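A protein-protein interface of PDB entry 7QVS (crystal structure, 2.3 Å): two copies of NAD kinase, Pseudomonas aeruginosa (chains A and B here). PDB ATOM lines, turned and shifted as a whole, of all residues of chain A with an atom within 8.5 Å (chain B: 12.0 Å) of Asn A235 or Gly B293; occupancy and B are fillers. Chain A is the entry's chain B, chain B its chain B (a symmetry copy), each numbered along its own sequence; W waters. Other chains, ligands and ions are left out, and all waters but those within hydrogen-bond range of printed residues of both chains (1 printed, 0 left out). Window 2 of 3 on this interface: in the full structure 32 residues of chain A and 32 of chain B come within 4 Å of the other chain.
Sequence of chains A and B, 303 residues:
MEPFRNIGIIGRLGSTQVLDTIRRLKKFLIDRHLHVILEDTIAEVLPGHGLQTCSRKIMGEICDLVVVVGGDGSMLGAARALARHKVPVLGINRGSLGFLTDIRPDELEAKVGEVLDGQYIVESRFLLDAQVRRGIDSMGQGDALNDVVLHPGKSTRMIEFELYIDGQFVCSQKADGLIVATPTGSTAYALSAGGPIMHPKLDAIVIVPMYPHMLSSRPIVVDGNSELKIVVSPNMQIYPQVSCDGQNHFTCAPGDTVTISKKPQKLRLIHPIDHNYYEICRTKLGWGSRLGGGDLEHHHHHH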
ATOM      1  N   GLU A 160       7.670   2.627 -31.318  1.00  0.00           N
ATOM      2  CA  GLU A 160       7.542   4.076 -31.381  1.00  0.00           C
ATOM      3  C   GLU A 160       8.451   4.697 -30.328  1.00  0.00           C
ATOM      4  O   GLU A 160       8.493   4.211 -29.199  1.00  0.00           O
ATOM      5  CB  GLU A 160       6.072   4.463 -31.182  1.00  0.00           C
ATOM      6  CG  GLU A 160       5.779   5.920 -31.306  1.00  0.00           C
ATOM      7  CD  GLU A 160       4.288   6.203 -31.310  1.00  0.00           C
ATOM      8  OE1 GLU A 160       3.625   5.983 -30.261  1.00  0.00           O
ATOM      9  OE2 GLU A 160       3.786   6.649 -32.365  1.00  0.00           O
ATOM     10  N   GLU A 162      11.033   8.492 -29.132  1.00  0.00           N
ATOM     11  CA  GLU A 162      11.511   9.857 -29.302  1.00  0.00           C
ATOM     12  C   GLU A 162      13.027   9.894 -29.174  1.00  0.00           C
ATOM     13  O   GLU A 162      13.621   9.103 -28.436  1.00  0.00           O
ATOM     14  CB  GLU A 162      10.881  10.812 -28.272  1.00  0.00           C
ATOM     15  CG  GLU A 162       9.393  11.063 -28.491  1.00  0.00           C
ATOM     16  CD  GLU A 162       8.738  11.845 -27.360  1.00  0.00           C
ATOM     17  OE1 GLU A 162       9.209  11.737 -26.200  1.00  0.00           O
ATOM     18  OE2 GLU A 162       7.755  12.578 -27.633  1.00  0.00           O
ATOM     19  N   VAL A 232      11.441   5.465 -25.032  1.00  0.00           N
ATOM     20  CA  VAL A 232      10.498   4.503 -25.583  1.00  0.00           C
ATOM     21  C   VAL A 232       9.088   5.000 -25.307  1.00  0.00           C
ATOM     22  O   VAL A 232       8.780   5.445 -24.194  1.00  0.00           O
ATOM     23  CB  VAL A 232      10.726   3.104 -24.981  1.00  0.00           C
ATOM     24  CG1 VAL A 232       9.686   2.134 -25.508  1.00  0.00           C
ATOM     25  CG2 VAL A 232      12.123   2.608 -25.282  1.00  0.00           C
ATOM     26  N   SER A 233       8.238   4.954 -26.325  1.00  0.00           N
ATOM     27  CA  SER A 233       6.917   5.562 -26.230  1.00  0.00           C
ATOM     28  C   SER A 233       6.125   4.974 -25.066  1.00  0.00           C
ATOM     29  O   SER A 233       6.035   3.746 -24.941  1.00  0.00           O
ATOM     30  CB  SER A 233       6.138   5.367 -27.521  1.00  0.00           C
ATOM     31  OG  SER A 233       4.787   5.726 -27.327  1.00  0.00           O
ATOM     32  N   PRO A 234       5.544   5.811 -24.197  1.00  0.00           N
ATOM     33  CA  PRO A 234       4.740   5.285 -23.088  1.00  0.00           C
ATOM     34  C   PRO A 234       3.409   4.696 -23.538  1.00  0.00           C
ATOM     35  O   PRO A 234       2.751   4.017 -22.739  1.00  0.00           O
ATOM     36  CB  PRO A 234       4.521   6.520 -22.198  1.00  0.00           C
ATOM     37  CG  PRO A 234       4.541   7.669 -23.152  1.00  0.00           C
ATOM     38  CD  PRO A 234       5.560   7.287 -24.220  1.00  0.00           C
ATOM     39  N   ASN A 235       2.987   4.944 -24.774  1.00  0.00           N
ATOM     40  CA  ASN A 235       1.735   4.408 -25.300  1.00  0.00           C
ATOM     41  C   ASN A 235       1.901   3.055 -25.975  1.00  0.00           C
ATOM     42  O   ASN A 235       0.932   2.544 -26.543  1.00  0.00           O
ATOM     43  CB  ASN A 235       1.116   5.381 -26.300  1.00  0.00           C
ATOM     44  CG  ASN A 235       0.960   6.753 -25.721  1.00  0.00           C
ATOM     45  OD1 ASN A 235       0.641   6.900 -24.534  1.00  0.00           O
ATOM     46  ND2 ASN A 235       1.220   7.775 -26.535  1.00  0.00           N
ATOM     47  N   MET A 236       3.094   2.473 -25.939  1.00  0.00           N
ATOM     48  CA  MET A 236       3.290   1.148 -26.498  1.00  0.00           C
ATOM     49  C   MET A 236       2.774   0.065 -25.566  1.00  0.00           C
ATOM     50  O   MET A 236       2.733   0.222 -24.343  1.00  0.00           O
ATOM     51  CB  MET A 236       4.760   0.860 -26.781  1.00  0.00           C
ATOM     52  CG  MET A 236       5.118   0.904 -28.249  1.00  0.00           C
ATOM     53  SD  MET A 236       6.844   1.240 -28.441  1.00  0.00           S
ATOM     54  CE  MET A 236       7.511  -0.378 -28.070  1.00  0.00           C
ATOM     55  N   GLN A 237       2.419  -1.058 -26.170  1.00  0.00           N
ATOM     56  CA  GLN A 237       1.958  -2.228 -25.450  1.00  0.00           C
ATOM     57  C   GLN A 237       3.003  -3.330 -25.374  1.00  0.00           C
ATOM     58  O   GLN A 237       2.787  -4.310 -24.662  1.00  0.00           O
ATOM     59  CB  GLN A 237       0.691  -2.773 -26.113  1.00  0.00           C
ATOM     60  CG  GLN A 237      -0.492  -1.819 -26.076  1.00  0.00           C
ATOM     61  CD  GLN A 237      -0.910  -1.471 -24.655  1.00  0.00           C
ATOM     62  OE1 GLN A 237      -1.101  -0.303 -24.322  1.00  0.00           O
ATOM     63  NE2 GLN A 237      -1.060  -2.487 -23.814  1.00  0.00           N
ATOM     64  N   ILE A 238       4.119  -3.204 -26.088  1.00  0.00           N
ATOM     65  CA  ILE A 238       5.150  -4.232 -26.099  1.00  0.00           C
ATOM     66  C   ILE A 238       6.441  -3.660 -25.524  1.00  0.00           C
ATOM     67  O   ILE A 238       6.663  -2.448 -25.491  1.00  0.00           O
ATOM     68  CB  ILE A 238       5.381  -4.827 -27.512  1.00  0.00           C
ATOM     69  CG1 ILE A 238       6.019  -3.796 -28.455  1.00  0.00           C
ATOM     70  CG2 ILE A 238       4.079  -5.384 -28.077  1.00  0.00           C
ATOM     71  CD1 ILE A 238       7.482  -4.091 -28.807  1.00  0.00           C
ATOM     72  N   ALA A 253      10.736  -1.226 -20.976  1.00  0.00           N
ATOM     73  CA  ALA A 253       9.323  -0.984 -20.784  1.00  0.00           C
ATOM     74  C   ALA A 253       8.921   0.327 -21.456  1.00  0.00           C
ATOM     75  O   ALA A 253       9.758   1.217 -21.640  1.00  0.00           O
ATOM     76  CB  ALA A 253       8.989  -0.927 -19.287  1.00  0.00           C
ATOM     77  N   PRO A 254       7.654   0.444 -21.854  1.00  0.00           N
ATOM     78  CA  PRO A 254       7.145   1.724 -22.354  1.00  0.00           C
ATOM     79  C   PRO A 254       7.462   2.849 -21.384  1.00  0.00           C
ATOM     80  O   PRO A 254       7.209   2.746 -20.186  1.00  0.00           O
ATOM     81  CB  PRO A 254       5.635   1.479 -22.455  1.00  0.00           C
ATOM     82  CG  PRO A 254       5.532   0.008 -22.697  1.00  0.00           C
ATOM     83  CD  PRO A 254       6.624  -0.610 -21.891  1.00  0.00           C
ATOM     84  N   GLY A 255       8.057   3.919 -21.905  1.00  0.00           N
ATOM     85  CA  GLY A 255       8.451   5.036 -21.083  1.00  0.00           C
ATOM     86  C   GLY A 255       9.882   5.006 -20.582  1.00  0.00           C
ATOM     87  O   GLY A 255      10.347   6.027 -20.060  1.00  0.00           O
ATOM     88  N   SER B 289       6.639  14.946 -34.588  1.00  0.00           N
ATOM     89  CA  SER B 289       6.764  15.835 -33.448  1.00  0.00           C
ATOM     90  C   SER B 289       6.598  15.042 -32.141  1.00  0.00           C
ATOM     91  O   SER B 289       6.508  13.815 -32.150  1.00  0.00           O
ATOM     92  CB  SER B 289       5.747  16.965 -33.572  1.00  0.00           C
ATOM     93  OG  SER B 289       4.439  16.430 -33.522  1.00  0.00           O
ATOM     94  N   ARG B 290       6.567  15.741 -31.000  1.00  0.00           N
ATOM     95  CA  ARG B 290       6.480  15.049 -29.719  1.00  0.00           C
ATOM     96  C   ARG B 290       5.225  14.173 -29.673  1.00  0.00           C
ATOM     97  O   ARG B 290       4.187  14.517 -30.246  1.00  0.00           O
ATOM     98  CB  ARG B 290       6.495  16.054 -28.557  1.00  0.00           C
ATOM     99  CG  ARG B 290       7.903  16.623 -28.199  1.00  0.00           C
ATOM    100  CD  ARG B 290       7.827  17.852 -27.251  1.00  0.00           C
ATOM    101  NE  ARG B 290       9.104  18.558 -27.113  1.00  0.00           N
ATOM    102  CZ  ARG B 290       9.556  19.480 -27.961  1.00  0.00           C
ATOM    103  NH1 ARG B 290       8.890  19.798 -29.061  1.00  0.00           N
ATOM    104  NH2 ARG B 290      10.710  20.096 -27.703  1.00  0.00           N
ATOM    105  N   LEU B 291       5.345  13.007 -29.038  1.00  0.00           N
ATOM    106  CA  LEU B 291       4.233  12.067 -28.968  1.00  0.00           C
ATOM    107  C   LEU B 291       3.091  12.629 -28.124  1.00  0.00           C
ATOM    108  O   LEU B 291       3.296  13.464 -27.243  1.00  0.00           O
ATOM    109  CB  LEU B 291       4.691  10.732 -28.392  1.00  0.00           C
ATOM    110  CG  LEU B 291       5.733   9.970 -29.209  1.00  0.00           C
ATOM    111  CD1 LEU B 291       6.156   8.733 -28.475  1.00  0.00           C
ATOM    112  CD2 LEU B 291       5.146   9.605 -30.547  1.00  0.00           C
ATOM    113  N   GLY B 292       1.872  12.164 -28.419  1.00  0.00           N
ATOM    114  CA  GLY B 292       0.676  12.534 -27.676  1.00  0.00           C
ATOM    115  C   GLY B 292       0.140  11.393 -26.831  1.00  0.00           C
ATOM    116  O   GLY B 292       0.920  10.563 -26.365  1.00  0.00           O
ATOM    117  N   GLY B 293      -1.175  11.327 -26.621  1.00  0.00           N
ATOM    118  CA  GLY B 293      -1.772  10.288 -25.792  1.00  0.00           C
ATOM    119  C   GLY B 293      -2.331   9.084 -26.529  1.00  0.00           C
ATOM    120  O   GLY B 293      -1.960   8.816 -27.683  1.00  0.00           O
HETATM  121  O   HOH W   1       5.919  13.495 -25.696  1.00  0.00           O
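Water W1 bridges the side-chain carboxylate of Glu A162 (2.8 Å) and the backbone carbonyl oxygen of Leu B291 (3.0 Å).
O of Glu A160 sits at hydrogen-bond distance from N of Ser A233 (3.0 Å). N of Glu A160 lies within hydrogen-bond range of SD of Met A236 (3.3 Å). The side-chain hydroxyl (OG) of Ser A233 lies close to the backbone NH (N) of Asn A235 (3.2 Å).
No position is printed for both chains.
OE2 of Glu A162 sits at hydrogen-bond distance from N of Leu B291 (2.8 Å). ND2 of Asn A235 sits at hydrogen-bond distance from O of Gly B292 (2.8 Å).
Printed residues of chain B that touch a printed residue of chain A: Arg B290, Leu B291, Gly B292 and Gly B293. Hydrophobic or aromatic side chains of chain B that line the printed part of chain A: Leu B291. Of the 12 printed residues of chain A, 4 touch a printed residue of chain B. Printed residues of chain A that touch a printed residue of chain B: Glu A160, Glu A162, Ser A233 and Asn A235. Among the printed residues, no Asp or Glu carboxylate lies within 4 Å of a Lys or Arg side-chain nitrogen of the other chain.
Of chain B, only Gly B292 (2.8 Å) and Gly B293 (3.5 Å) come within 4 Å of Asn A235. Of the printed residues of chain A, Gly B293 touches Asn A235 (3.5 Å). Of chain B, only Leu B291 comes within 4 Å of Ser A233. No residue of chain B comes within 4 Å of Pro A234. No residue of chain B comes within 4 Å of Met A236. No residue of chain B comes within 4 Å of Gln A237. Gly B292 touches one residue of chain A. Printed residues of chain A within 4 Å of Arg B290: Glu A162 (3.5 Å). Of the printed residues of chain B, Glu A162 touches Arg B290 and Leu B291. Of the printed residues of chain A, Leu B291 touches Glu A160 (3.6 Å), Glu A162 (2.8 Å) and Ser A233 (3.5 Å). Gly A255 touches none of the printed residues of chain B. Ala A253 touches none of the printed residues of chain B. The nearest residue of chain A that does not touch Gly B293 is Glu A160 (6.8 Å). The nearest printed residue of chain A that does not touch Leu B291 is Pro A234 (4.5 Å).
Glu A160 touches Leu B291. OE2 of Glu A162 touches CA of Arg B290 (3.5 Å). Ser A233 touches Leu B291 (OG to CD1, 3.5 Å). Asn A235 touches Gly B293 (ND2 to O, 3.5 Å).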
